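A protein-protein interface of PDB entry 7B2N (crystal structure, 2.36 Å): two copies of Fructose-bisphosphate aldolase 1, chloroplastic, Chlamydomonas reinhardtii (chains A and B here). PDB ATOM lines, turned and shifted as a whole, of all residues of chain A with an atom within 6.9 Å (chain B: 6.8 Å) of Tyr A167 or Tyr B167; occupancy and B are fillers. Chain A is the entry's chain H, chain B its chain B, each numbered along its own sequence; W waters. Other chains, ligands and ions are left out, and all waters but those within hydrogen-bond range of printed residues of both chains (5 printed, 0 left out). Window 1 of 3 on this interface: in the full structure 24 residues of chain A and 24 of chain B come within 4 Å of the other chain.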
ATOM      1  N   LEU A 115      -4.849  10.451   6.225  1.00  0.00           N
ATOM      2  CA  LEU A 115      -5.616  11.489   5.553  1.00  0.00           C
ATOM      3  C   LEU A 115      -5.710  12.702   6.465  1.00  0.00           C
ATOM      4  O   LEU A 115      -6.042  12.569   7.647  1.00  0.00           O
ATOM      5  CB  LEU A 115      -7.016  10.988   5.186  1.00  0.00           C
ATOM      6  CG  LEU A 115      -7.946  12.003   4.513  1.00  0.00           C
ATOM      7  CD1 LEU A 115      -7.298  12.574   3.261  1.00  0.00           C
ATOM      8  CD2 LEU A 115      -9.294  11.370   4.171  1.00  0.00           C
ATOM      9  N   LEU A 127      -1.868   8.151  -7.760  1.00  0.00           N
ATOM     10  CA  LEU A 127      -2.291   8.711  -9.042  1.00  0.00           C
ATOM     11  C   LEU A 127      -1.137   9.376  -9.784  1.00  0.00           C
ATOM     12  O   LEU A 127      -1.092   9.333 -11.020  1.00  0.00           O
ATOM     13  CB  LEU A 127      -3.435   9.703  -8.838  1.00  0.00           C
ATOM     14  CG  LEU A 127      -4.752   9.100  -8.343  1.00  0.00           C
ATOM     15  CD1 LEU A 127      -5.782  10.186  -8.093  1.00  0.00           C
ATOM     16  CD2 LEU A 127      -5.280   8.059  -9.323  1.00  0.00           C
ATOM     17  N   ILE A 160     -15.126  12.433   4.318  1.00  0.00           N
ATOM     18  CA  ILE A 160     -14.025  12.680   3.394  1.00  0.00           C
ATOM     19  C   ILE A 160     -13.145  11.446   3.226  1.00  0.00           C
ATOM     20  O   ILE A 160     -12.508  11.277   2.180  1.00  0.00           O
ATOM     21  CB  ILE A 160     -13.208  13.904   3.842  1.00  0.00           C
ATOM     22  CG1 ILE A 160     -12.579  13.667   5.218  1.00  0.00           C
ATOM     23  CG2 ILE A 160     -14.084  15.157   3.847  1.00  0.00           C
ATOM     24  CD1 ILE A 160     -11.562  14.716   5.603  1.00  0.00           C
ATOM     25  N   ALA A 161     -13.094  10.560   4.223  1.00  0.00           N
ATOM     26  CA  ALA A 161     -12.297   9.343   4.084  1.00  0.00           C
ATOM     27  C   ALA A 161     -12.933   8.380   3.089  1.00  0.00           C
ATOM     28  O   ALA A 161     -12.252   7.842   2.207  1.00  0.00           O
ATOM     29  CB  ALA A 161     -12.112   8.672   5.443  1.00  0.00           C
ATOM     30  N   ALA A 162     -14.241   8.135   3.226  1.00  0.00           N
ATOM     31  CA  ALA A 162     -14.942   7.310   2.248  1.00  0.00           C
ATOM     32  C   ALA A 162     -14.934   7.964   0.874  1.00  0.00           C
ATOM     33  O   ALA A 162     -14.823   7.277  -0.148  1.00  0.00           O
ATOM     34  CB  ALA A 162     -16.380   7.051   2.705  1.00  0.00           C
ATOM     35  N   ARG A 163     -15.050   9.295   0.833  1.00  0.00           N
ATOM     36  CA  ARG A 163     -15.049  10.003  -0.443  1.00  0.00           C
ATOM     37  C   ARG A 163     -13.755   9.758  -1.207  1.00  0.00           C
ATOM     38  O   ARG A 163     -13.780   9.388  -2.386  1.00  0.00           O
ATOM     39  CB  ARG A 163     -15.264  11.501  -0.220  1.00  0.00           C
ATOM     40  CG  ARG A 163     -15.246  12.328  -1.501  1.00  0.00           C
ATOM     41  CD  ARG A 163     -15.427  13.813  -1.215  1.00  0.00           C
ATOM     42  NE  ARG A 163     -16.740  14.104  -0.647  1.00  0.00           N
ATOM     43  CZ  ARG A 163     -17.040  15.216   0.017  1.00  0.00           C
ATOM     44  NH1 ARG A 163     -16.119  16.157   0.199  1.00  0.00           N
ATOM     45  NH2 ARG A 163     -18.262  15.391   0.499  1.00  0.00           N
ATOM     46  N   ASP A 164     -12.606   9.946  -0.548  1.00  0.00           N
ATOM     47  CA  ASP A 164     -11.334   9.782  -1.246  1.00  0.00           C
ATOM     48  C   ASP A 164     -11.088   8.337  -1.648  1.00  0.00           C
ATOM     49  O   ASP A 164     -10.469   8.087  -2.688  1.00  0.00           O
ATOM     50  CB  ASP A 164     -10.169  10.271  -0.391  1.00  0.00           C
ATOM     51  CG  ASP A 164      -8.888  10.405  -1.202  1.00  0.00           C
ATOM     52  OD1 ASP A 164      -8.767  11.403  -1.944  1.00  0.00           O
ATOM     53  OD2 ASP A 164      -8.025   9.502  -1.128  1.00  0.00           O
ATOM     54  N   CYS A 165     -11.535   7.384  -0.823  1.00  0.00           N
ATOM     55  CA  CYS A 165     -11.448   5.976  -1.185  1.00  0.00           C
ATOM     56  C   CYS A 165     -12.180   5.714  -2.496  1.00  0.00           C
ATOM     57  O   CYS A 165     -11.634   5.101  -3.419  1.00  0.00           O
ATOM     58  CB  CYS A 165     -12.034   5.122  -0.058  1.00  0.00           C
ATOM     59  SG  CYS A 165     -12.254   3.371  -0.443  1.00  0.00           S
ATOM     60  N   ALA A 166     -13.424   6.189  -2.596  1.00  0.00           N
ATOM     61  CA  ALA A 166     -14.189   6.047  -3.830  1.00  0.00           C
ATOM     62  C   ALA A 166     -13.648   6.954  -4.927  1.00  0.00           C
ATOM     63  O   ALA A 166     -13.609   6.557  -6.095  1.00  0.00           O
ATOM     64  CB  ALA A 166     -15.664   6.341  -3.560  1.00  0.00           C
ATOM     65  N   TYR A 167     -13.229   8.176  -4.578  1.00  0.00           N
ATOM     66  CA  TYR A 167     -12.743   9.098  -5.603  1.00  0.00           C
ATOM     67  C   TYR A 167     -11.439   8.609  -6.220  1.00  0.00           C
ATOM     68  O   TYR A 167     -11.274   8.651  -7.444  1.00  0.00           O
ATOM     69  CB  TYR A 167     -12.553  10.503  -5.028  1.00  0.00           C
ATOM     70  CG  TYR A 167     -12.187  11.536  -6.074  1.00  0.00           C
ATOM     71  CD1 TYR A 167     -13.168  12.146  -6.845  1.00  0.00           C
ATOM     72  CD2 TYR A 167     -10.859  11.894  -6.297  1.00  0.00           C
ATOM     73  CE1 TYR A 167     -12.843  13.085  -7.805  1.00  0.00           C
ATOM     74  CE2 TYR A 167     -10.522  12.835  -7.255  1.00  0.00           C
ATOM     75  CZ  TYR A 167     -11.523  13.427  -8.007  1.00  0.00           C
ATOM     76  OH  TYR A 167     -11.213  14.364  -8.966  1.00  0.00           O
ATOM     77  N   GLY A 168     -10.499   8.148  -5.391  1.00  0.00           N
ATOM     78  CA  GLY A 168      -9.241   7.657  -5.925  1.00  0.00           C
ATOM     79  C   GLY A 168      -9.416   6.422  -6.787  1.00  0.00           C
ATOM     80  O   GLY A 168      -8.814   6.309  -7.859  1.00  0.00           O
ATOM     81  N   LEU A 169     -10.247   5.478  -6.334  1.00  0.00           N
ATOM     82  CA  LEU A 169     -10.468   4.258  -7.105  1.00  0.00           C
ATOM     83  C   LEU A 169     -11.085   4.570  -8.463  1.00  0.00           C
ATOM     84  O   LEU A 169     -10.718   3.961  -9.475  1.00  0.00           O
ATOM     85  CB  LEU A 169     -11.351   3.292  -6.315  1.00  0.00           C
ATOM     86  CG  LEU A 169     -10.620   2.393  -5.313  1.00  0.00           C
ATOM     87  CD1 LEU A 169     -11.560   1.930  -4.218  1.00  0.00           C
ATOM     88  CD2 LEU A 169     -10.000   1.201  -6.022  1.00  0.00           C
ATOM     89  N   ALA A 170     -12.009   5.532  -8.510  1.00  0.00           N
ATOM     90  CA  ALA A 170     -12.609   5.899  -9.789  1.00  0.00           C
ATOM     91  C   ALA A 170     -11.609   6.617 -10.690  1.00  0.00           C
ATOM     92  O   ALA A 170     -11.650   6.450 -11.916  1.00  0.00           O
ATOM     93  CB  ALA A 170     -13.851   6.760  -9.568  1.00  0.00           C
ATOM     94  N   ARG A 171     -10.714   7.428 -10.110  1.00  0.00           N
ATOM     95  CA  ARG A 171      -9.643   8.029 -10.906  1.00  0.00           C
ATOM     96  C   ARG A 171      -8.718   6.950 -11.462  1.00  0.00           C
ATOM     97  O   ARG A 171      -8.416   6.931 -12.661  1.00  0.00           O
ATOM     98  CB  ARG A 171      -8.839   9.037 -10.071  1.00  0.00           C
ATOM     99  CG  ARG A 171      -9.563  10.332  -9.694  1.00  0.00           C
ATOM    100  CD  ARG A 171      -9.698  11.323 -10.854  1.00  0.00           C
ATOM    101  NE  ARG A 171      -8.521  11.378 -11.720  1.00  0.00           N
ATOM    102  CZ  ARG A 171      -7.437  12.112 -11.477  1.00  0.00           C
ATOM    103  NH1 ARG A 171      -7.360  12.860 -10.384  1.00  0.00           N
ATOM    104  NH2 ARG A 171      -6.421  12.093 -12.329  1.00  0.00           N
ATOM    105  N   TYR A 172      -8.266   6.035 -10.596  1.00  0.00           N
ATOM    106  CA  TYR A 172      -7.368   4.966 -11.028  1.00  0.00           C
ATOM    107  C   TYR A 172      -8.010   4.098 -12.107  1.00  0.00           C
ATOM    108  O   TYR A 172      -7.364   3.765 -13.108  1.00  0.00           O
ATOM    109  CB  TYR A 172      -6.956   4.122  -9.820  1.00  0.00           C
ATOM    110  CG  TYR A 172      -6.891   2.628 -10.073  1.00  0.00           C
ATOM    111  CD1 TYR A 172      -5.827   2.064 -10.765  1.00  0.00           C
ATOM    112  CD2 TYR A 172      -7.897   1.783  -9.614  1.00  0.00           C
ATOM    113  CE1 TYR A 172      -5.767   0.702 -10.994  1.00  0.00           C
ATOM    114  CE2 TYR A 172      -7.845   0.416  -9.839  1.00  0.00           C
ATOM    115  CZ  TYR A 172      -6.777  -0.118 -10.527  1.00  0.00           C
ATOM    116  OH  TYR A 172      -6.725  -1.474 -10.752  1.00  0.00           O
ATOM    117  N   GLU A 210     -21.070   5.051  -3.815  1.00  0.00           N
ATOM    118  CA  GLU A 210     -20.198   6.189  -4.081  1.00  0.00           C
ATOM    119  C   GLU A 210     -19.160   5.852  -5.143  1.00  0.00           C
ATOM    120  O   GLU A 210     -18.882   6.669  -6.029  1.00  0.00           O
ATOM    121  CB  GLU A 210     -19.523   6.637  -2.787  1.00  0.00           C
ATOM    122  CG  GLU A 210     -19.007   8.062  -2.819  1.00  0.00           C
ATOM    123  CD  GLU A 210     -18.535   8.543  -1.457  1.00  0.00           C
ATOM    124  OE1 GLU A 210     -18.597   7.757  -0.487  1.00  0.00           O
ATOM    125  OE2 GLU A 210     -18.102   9.711  -1.361  1.00  0.00           O
ATOM    126  N   THR A 211     -18.582   4.652  -5.079  1.00  0.00           N
ATOM    127  CA  THR A 211     -17.546   4.284  -6.039  1.00  0.00           C
ATOM    128  C   THR A 211     -18.111   4.167  -7.449  1.00  0.00           C
ATOM    129  O   THR A 211     -17.492   4.637  -8.412  1.00  0.00           O
ATOM    130  CB  THR A 211     -16.882   2.976  -5.612  1.00  0.00           C
ATOM    131  OG1 THR A 211     -16.377   3.113  -4.278  1.00  0.00           O
ATOM    132  CG2 THR A 211     -15.738   2.628  -6.544  1.00  0.00           C
ATOM    133  N   TYR A 214     -18.916   7.752  -8.962  1.00  0.00           N
ATOM    134  CA  TYR A 214     -17.728   8.429  -9.472  1.00  0.00           C
ATOM    135  C   TYR A 214     -17.207   7.755 -10.737  1.00  0.00           C
ATOM    136  O   TYR A 214     -16.793   8.435 -11.685  1.00  0.00           O
ATOM    137  CB  TYR A 214     -16.638   8.469  -8.401  1.00  0.00           C
ATOM    138  CG  TYR A 214     -16.789   9.576  -7.380  1.00  0.00           C
ATOM    139  CD1 TYR A 214     -17.053  10.883  -7.774  1.00  0.00           C
ATOM    140  CD2 TYR A 214     -16.660   9.315  -6.021  1.00  0.00           C
ATOM    141  CE1 TYR A 214     -17.186  11.898  -6.842  1.00  0.00           C
ATOM    142  CE2 TYR A 214     -16.791  10.323  -5.083  1.00  0.00           C
ATOM    143  CZ  TYR A 214     -17.057  11.610  -5.502  1.00  0.00           C
ATOM    144  OH  TYR A 214     -17.197  12.612  -4.576  1.00  0.00           O
ATOM    145  N   ASN A 218     -16.656   9.366 -14.417  1.00  0.00           N
ATOM    146  CA  ASN A 218     -15.376   9.280 -15.105  1.00  0.00           C
ATOM    147  C   ASN A 218     -15.447   8.489 -16.405  1.00  0.00           C
ATOM    148  O   ASN A 218     -14.403   8.270 -17.033  1.00  0.00           O
ATOM    149  CB  ASN A 218     -14.324   8.665 -14.182  1.00  0.00           C
ATOM    150  CG  ASN A 218     -13.990   9.555 -13.005  1.00  0.00           C
ATOM    151  OD1 ASN A 218     -14.415  10.708 -12.940  1.00  0.00           O
ATOM    152  ND2 ASN A 218     -13.220   9.023 -12.066  1.00  0.00           N
ATOM    153  N   LEU B 115      -6.144  14.670 -18.139  1.00  0.00           N
ATOM    154  CA  LEU B 115      -7.145  13.968 -17.353  1.00  0.00           C
ATOM    155  C   LEU B 115      -7.855  12.942 -18.227  1.00  0.00           C
ATOM    156  O   LEU B 115      -8.361  13.275 -19.305  1.00  0.00           O
ATOM    157  CB  LEU B 115      -8.145  14.967 -16.773  1.00  0.00           C
ATOM    158  CG  LEU B 115      -9.251  14.423 -15.883  1.00  0.00           C
ATOM    159  CD1 LEU B 115      -8.674  13.568 -14.772  1.00  0.00           C
ATOM    160  CD2 LEU B 115     -10.040  15.583 -15.313  1.00  0.00           C
ATOM    161  N   LEU B 127      -0.220  15.104  -5.019  1.00  0.00           N
ATOM    162  CA  LEU B 127      -0.598  14.713  -3.663  1.00  0.00           C
ATOM    163  C   LEU B 127       0.302  13.611  -3.112  1.00  0.00           C
ATOM    164  O   LEU B 127       0.501  13.530  -1.894  1.00  0.00           O
ATOM    165  CB  LEU B 127      -2.062  14.272  -3.627  1.00  0.00           C
ATOM    166  CG  LEU B 127      -3.084  15.334  -4.032  1.00  0.00           C
ATOM    167  CD1 LEU B 127      -4.501  14.765  -4.025  1.00  0.00           C
ATOM    168  CD2 LEU B 127      -2.984  16.544  -3.122  1.00  0.00           C
ATOM    169  N   ILE B 160     -15.972  16.627 -14.476  1.00  0.00           N
ATOM    170  CA  ILE B 160     -14.905  15.930 -13.761  1.00  0.00           C
ATOM    171  C   ILE B 160     -13.607  16.728 -13.784  1.00  0.00           C
ATOM    172  O   ILE B 160     -12.795  16.626 -12.855  1.00  0.00           O
ATOM    173  CB  ILE B 160     -14.706  14.511 -14.324  1.00  0.00           C
ATOM    174  CG1 ILE B 160     -14.277  14.562 -15.791  1.00  0.00           C
ATOM    175  CG2 ILE B 160     -15.979  13.690 -14.152  1.00  0.00           C
ATOM    176  CD1 ILE B 160     -13.902  13.210 -16.351  1.00  0.00           C
ATOM    177  N   ALA B 161     -13.377  17.532 -14.823  1.00  0.00           N
ATOM    178  CA  ALA B 161     -12.197  18.392 -14.826  1.00  0.00           C
ATOM    179  C   ALA B 161     -12.308  19.474 -13.763  1.00  0.00           C
ATOM    180  O   ALA B 161     -11.347  19.744 -13.031  1.00  0.00           O
ATOM    181  CB  ALA B 161     -11.987  19.013 -16.205  1.00  0.00           C
ATOM    182  N   ALA B 162     -13.471  20.122 -13.671  1.00  0.00           N
ATOM    183  CA  ALA B 162     -13.660  21.126 -12.631  1.00  0.00           C
ATOM    184  C   ALA B 162     -13.615  20.491 -11.250  1.00  0.00           C
ATOM    185  O   ALA B 162     -13.067  21.078 -10.308  1.00  0.00           O
ATOM    186  CB  ALA B 162     -14.980  21.867 -12.845  1.00  0.00           C
ATOM    187  N   ARG B 163     -14.168  19.282 -11.114  1.00  0.00           N
ATOM    188  CA  ARG B 163     -14.177  18.613  -9.816  1.00  0.00           C
ATOM    189  C   ARG B 163     -12.764  18.327  -9.331  1.00  0.00           C
ATOM    190  O   ARG B 163     -12.437  18.577  -8.166  1.00  0.00           O
ATOM    191  CB  ARG B 163     -14.991  17.320  -9.885  1.00  0.00           C
ATOM    192  CG  ARG B 163     -15.037  16.556  -8.566  1.00  0.00           C
ATOM    193  CD  ARG B 163     -15.836  15.273  -8.696  1.00  0.00           C
ATOM    194  NE  ARG B 163     -17.242  15.533  -8.987  1.00  0.00           N
ATOM    195  CZ  ARG B 163     -18.027  14.718  -9.685  1.00  0.00           C
ATOM    196  NH1 ARG B 163     -17.544  13.583 -10.176  1.00  0.00           N
ATOM    197  NH2 ARG B 163     -19.299  15.038  -9.894  1.00  0.00           N
ATOM    198  N   ASP B 164     -11.902  17.807 -10.207  1.00  0.00           N
ATOM    199  CA  ASP B 164     -10.569  17.418  -9.742  1.00  0.00           C
ATOM    200  C   ASP B 164      -9.729  18.630  -9.363  1.00  0.00           C
ATOM    201  O   ASP B 164      -8.935  18.562  -8.415  1.00  0.00           O
ATOM    202  CB  ASP B 164      -9.847  16.586 -10.790  1.00  0.00           C
ATOM    203  CG  ASP B 164      -8.606  15.933 -10.222  1.00  0.00           C
ATOM    204  OD1 ASP B 164      -8.757  14.939  -9.481  1.00  0.00           O
ATOM    205  OD2 ASP B 164      -7.487  16.434 -10.480  1.00  0.00           O
ATOM    206  N   CYS B 165      -9.883  19.728 -10.116  1.00  0.00           N
ATOM    207  CA  CYS B 165      -9.226  20.992  -9.812  1.00  0.00           C
ATOM    208  C   CYS B 165      -9.609  21.486  -8.412  1.00  0.00           C
ATOM    209  O   CYS B 165      -8.756  21.882  -7.614  1.00  0.00           O
ATOM    210  CB  CYS B 165      -9.635  22.026 -10.868  1.00  0.00           C
ATOM    211  SG  CYS B 165      -9.405  23.780 -10.444  1.00  0.00           S
ATOM    212  N   ALA B 166     -10.907  21.521  -8.127  1.00  0.00           N
ATOM    213  CA  ALA B 166     -11.389  21.914  -6.807  1.00  0.00           C
ATOM    214  C   ALA B 166     -11.015  20.876  -5.758  1.00  0.00           C
ATOM    215  O   ALA B 166     -10.621  21.234  -4.644  1.00  0.00           O
ATOM    216  CB  ALA B 166     -12.904  22.114  -6.872  1.00  0.00           C
ATOM    217  N   TYR B 167     -11.125  19.590  -6.098  1.00  0.00           N
ATOM    218  CA  TYR B 167     -10.878  18.538  -5.115  1.00  0.00           C
ATOM    219  C   TYR B 167      -9.397  18.431  -4.768  1.00  0.00           C
ATOM    220  O   TYR B 167      -9.046  18.245  -3.598  1.00  0.00           O
ATOM    221  CB  TYR B 167     -11.405  17.202  -5.637  1.00  0.00           C
ATOM    222  CG  TYR B 167     -11.308  16.065  -4.647  1.00  0.00           C
ATOM    223  CD1 TYR B 167     -12.288  15.873  -3.676  1.00  0.00           C
ATOM    224  CD2 TYR B 167     -10.233  15.183  -4.679  1.00  0.00           C
ATOM    225  CE1 TYR B 167     -12.200  14.836  -2.770  1.00  0.00           C
ATOM    226  CE2 TYR B 167     -10.133  14.144  -3.775  1.00  0.00           C
ATOM    227  CZ  TYR B 167     -11.117  13.976  -2.823  1.00  0.00           C
ATOM    228  OH  TYR B 167     -11.019  12.945  -1.922  1.00  0.00           O
ATOM    229  N   GLY B 168      -8.516  18.523  -5.767  1.00  0.00           N
ATOM    230  CA  GLY B 168      -7.092  18.442  -5.489  1.00  0.00           C
ATOM    231  C   GLY B 168      -6.593  19.638  -4.699  1.00  0.00           C
ATOM    232  O   GLY B 168      -5.781  19.494  -3.780  1.00  0.00           O
ATOM    233  N   LEU B 169      -7.079  20.832  -5.042  1.00  0.00           N
ATOM    234  CA  LEU B 169      -6.711  22.030  -4.298  1.00  0.00           C
ATOM    235  C   LEU B 169      -7.115  21.914  -2.833  1.00  0.00           C
ATOM    236  O   LEU B 169      -6.329  22.227  -1.932  1.00  0.00           O
ATOM    237  CB  LEU B 169      -7.354  23.255  -4.943  1.00  0.00           C
ATOM    238  CG  LEU B 169      -6.524  23.863  -6.073  1.00  0.00           C
ATOM    239  CD1 LEU B 169      -7.408  24.682  -6.978  1.00  0.00           C
ATOM    240  CD2 LEU B 169      -5.403  24.716  -5.506  1.00  0.00           C
ATOM    241  N   ALA B 170      -8.339  21.449  -2.574  1.00  0.00           N
ATOM    242  CA  ALA B 170      -8.794  21.333  -1.191  1.00  0.00           C
ATOM    243  C   ALA B 170      -8.028  20.261  -0.425  1.00  0.00           C
ATOM    244  O   ALA B 170      -7.801  20.411   0.781  1.00  0.00           O
ATOM    245  CB  ALA B 170     -10.290  21.036  -1.150  1.00  0.00           C
ATOM    246  N   ARG B 171      -7.637  19.175  -1.092  1.00  0.00           N
ATOM    247  CA  ARG B 171      -6.822  18.169  -0.425  1.00  0.00           C
ATOM    248  C   ARG B 171      -5.427  18.699  -0.144  1.00  0.00           C
ATOM    249  O   ARG B 171      -4.892  18.508   0.952  1.00  0.00           O
ATOM    250  CB  ARG B 171      -6.753  16.906  -1.275  1.00  0.00           C
ATOM    251  CG  ARG B 171      -8.034  16.120  -1.247  1.00  0.00           C
ATOM    252  CD  ARG B 171      -7.963  15.041  -0.207  1.00  0.00           C
ATOM    253  NE  ARG B 171      -7.389  13.845  -0.797  1.00  0.00           N
ATOM    254  CZ  ARG B 171      -6.237  13.305  -0.429  1.00  0.00           C
ATOM    255  NH1 ARG B 171      -5.516  13.835   0.553  1.00  0.00           N
ATOM    256  NH2 ARG B 171      -5.813  12.223  -1.049  1.00  0.00           N
ATOM    257  N   TYR B 172      -4.844  19.398  -1.105  1.00  0.00           N
ATOM    258  CA  TYR B 172      -3.493  19.970  -0.958  1.00  0.00           C
ATOM    259  C   TYR B 172      -3.500  21.011   0.165  1.00  0.00           C
ATOM    260  O   TYR B 172      -2.561  21.088   0.902  1.00  0.00           O
ATOM    261  CB  TYR B 172      -3.019  20.545  -2.292  1.00  0.00           C
ATOM    262  CG  TYR B 172      -2.392  21.906  -2.193  1.00  0.00           C
ATOM    263  CD1 TYR B 172      -1.048  22.049  -1.941  1.00  0.00           C
ATOM    264  CD2 TYR B 172      -3.145  23.043  -2.301  1.00  0.00           C
ATOM    265  CE1 TYR B 172      -0.459  23.283  -1.807  1.00  0.00           C
ATOM    266  CE2 TYR B 172      -2.581  24.284  -2.165  1.00  0.00           C
ATOM    267  CZ  TYR B 172      -1.226  24.410  -1.938  1.00  0.00           C
ATOM    268  OH  TYR B 172      -0.660  25.623  -1.816  1.00  0.00           O
ATOM    269  N   GLU B 210     -17.178  25.502  -5.650  1.00  0.00           N
ATOM    270  CA  GLU B 210     -16.805  24.102  -5.499  1.00  0.00           C
ATOM    271  C   GLU B 210     -15.552  23.960  -4.642  1.00  0.00           C
ATOM    272  O   GLU B 210     -15.511  23.143  -3.717  1.00  0.00           O
ATOM    273  CB  GLU B 210     -16.599  23.465  -6.873  1.00  0.00           C
ATOM    274  CG  GLU B 210     -16.714  21.946  -6.869  1.00  0.00           C
ATOM    275  CD  GLU B 210     -16.594  21.336  -8.259  1.00  0.00           C
ATOM    276  OE1 GLU B 210     -16.512  22.096  -9.257  1.00  0.00           O
ATOM    277  OE2 GLU B 210     -16.584  20.089  -8.352  1.00  0.00           O
ATOM    278  N   THR B 211     -14.519  24.753  -4.938  1.00  0.00           N
ATOM    279  CA  THR B 211     -13.276  24.673  -4.177  1.00  0.00           C
ATOM    280  C   THR B 211     -13.507  24.969  -2.701  1.00  0.00           C
ATOM    281  O   THR B 211     -12.919  24.316  -1.830  1.00  0.00           O
ATOM    282  CB  THR B 211     -12.244  25.642  -4.761  1.00  0.00           C
ATOM    283  OG1 THR B 211     -12.038  25.341  -6.151  1.00  0.00           O
ATOM    284  CG2 THR B 211     -10.919  25.530  -4.015  1.00  0.00           C
ATOM    285  N   TYR B 214     -15.346  21.882  -0.919  1.00  0.00           N
ATOM    286  CA  TYR B 214     -14.411  20.809  -0.605  1.00  0.00           C
ATOM    287  C   TYR B 214     -13.482  21.199   0.542  1.00  0.00           C
ATOM    288  O   TYR B 214     -13.210  20.382   1.427  1.00  0.00           O
ATOM    289  CB  TYR B 214     -13.615  20.430  -1.854  1.00  0.00           C
ATOM    290  CG  TYR B 214     -14.376  19.530  -2.807  1.00  0.00           C
ATOM    291  CD1 TYR B 214     -15.093  18.438  -2.336  1.00  0.00           C
ATOM    292  CD2 TYR B 214     -14.382  19.777  -4.172  1.00  0.00           C
ATOM    293  CE1 TYR B 214     -15.791  17.615  -3.197  1.00  0.00           C
ATOM    294  CE2 TYR B 214     -15.074  18.957  -5.043  1.00  0.00           C
ATOM    295  CZ  TYR B 214     -15.778  17.879  -4.551  1.00  0.00           C
ATOM    296  OH  TYR B 214     -16.471  17.064  -5.418  1.00  0.00           O
ATOM    297  N   ASN B 218     -12.977  19.411   4.147  1.00  0.00           N
ATOM    298  CA  ASN B 218     -11.671  18.957   4.604  1.00  0.00           C
ATOM    299  C   ASN B 218     -11.202  19.667   5.868  1.00  0.00           C
ATOM    300  O   ASN B 218     -10.059  19.448   6.287  1.00  0.00           O
ATOM    301  CB  ASN B 218     -10.635  19.146   3.491  1.00  0.00           C
ATOM    302  CG  ASN B 218     -10.897  18.249   2.296  1.00  0.00           C
ATOM    303  OD1 ASN B 218     -11.707  17.325   2.366  1.00  0.00           O
ATOM    304  ND2 ASN B 218     -10.209  18.519   1.188  1.00  0.00           N
HETATM  305  O   HOH W   1     -18.001  15.181  -4.882  1.00  0.00           O
HETATM  306  O   HOH W   2     -12.679  13.979 -11.311  1.00  0.00           O
HETATM  307  O   HOH W   3     -13.359  16.017   0.208  1.00  0.00           O
HETATM  308  O   HOH W   4     -15.067  12.503 -10.577  1.00  0.00           O
HETATM  309  O   HOH W   5     -11.808  13.550   0.380  1.00  0.00           O
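Leu A115 touches Arg B171, and with the chains exchanged Arg A171 touches Leu B115. Arg A163 touches Tyr B214, and with the chains exchanged Tyr A214 touches Arg B163. Of the 13 pairs that touch across the chains among the printed residues, 13 have their exchanged pair printed and touching as well.
The side-chain carboxylate (OD1) of Asp B164 is in hydrogen-bond range of the side-chain hydroxyl (OH) of Tyr A167 (2.6 Å). The side-chain carboxylate (OD1) of Asp B164 is in salt-bridge range of the guanidinium group (NH1) of Arg A171, 2.7 Å away. The side-chain carboxylate (OD1) of Asp A164 sits at hydrogen-bond distance from the side-chain hydroxyl (OH) of Tyr B167, 2.7 Å away. The side-chain carboxylate (OD1) of Asp A164 is in salt-bridge range of the guanidinium group (NE) of Arg B171 (3.0 Å).
Arg B171 touches Leu A115. Ile A160 touches Asn B218 (CG2 to OD1, 3.5 Å). CD of Arg A163 touches CE1 of Tyr B167 (3.7 Å). CD1 of Tyr B214 touches NH1 of Arg A163, at 3.6 Å. Tyr A167 touches Arg B163 (CE1 to CD, 3.8 Å). Tyr B167 touches Tyr A167. Arg A171 touches Leu B115 (NH2 to CD1, 3.6 Å). Arg B163 touches Tyr A214. Ile B160 touches Asn A218 (CG2 to OD1, 3.6 Å).
The backbone carbonyl oxygen of Ala B170 sits at hydrogen-bond distance from the side-chain amide nitrogen of Asn B218, at 3.1 Å. The side-chain amide nitrogen of Asn B218 lies close to the backbone NH of Arg B171. The backbone carbonyl oxygen of Ala A170 lies within hydrogen-bond range of the side-chain amide nitrogen of Asn A218 (3.0 Å).
Of chain B, only Arg B163 (3.8 Å), Asp B164 (2.6 Å) and Tyr B167 (3.5 Å) come within 4 Å of Tyr A167. Of chain A, only Arg A163, Asp A164 and Tyr A167 come within 4 Å of Tyr B167. Printed residues of chain A within 4 Å of Leu B115: Arg A171. Printed residues of chain B within 4 Å of Asp A164: Tyr B167 and Arg B171. The nearest residue of chain A that does not touch Tyr B167 is Ile A160 (4.7 Å). The nearest printed residue of chain A that does not touch Leu B115 is Tyr A167 (6.4 Å).
Water W5 lies within hydrogen-bond range of the side-chain hydroxyl of Tyr B167 (2.5 Å) and the backbone carbonyl oxygen of Ile A160 (3.0 Å). Water W2 lies within hydrogen-bond range of the side-chain hydroxyl of Tyr A167 (2.8 Å) and the backbone carbonyl oxygen of Ile B160 (3.1 Å).
Of the 19 printed residues of chain B, 8 touch a printed residue of chain A. Hydrophobic or aromatic side chains of chain B within 4 Å of the printed part of chain A: Leu B115, Ile B160, Tyr B167 and Tyr B214. Along chain B the printed residues that touch a printed residue of chain A span positions 115 to 218. Hydrophobic or aromatic side chains of chain A that line the printed part of chain B: Leu A115, Ile A160, Tyr A167 and Tyr A214. Among the printed residues, 13 pairs touch across the chains. Among the printed residues, Asp or Glu carboxylates within 4 Å of a Lys or Arg side-chain nitrogen of the other chain: Asp A164 with Arg B171 (3.0 Å) and Arg A171 with Asp B164 (2.7 Å).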
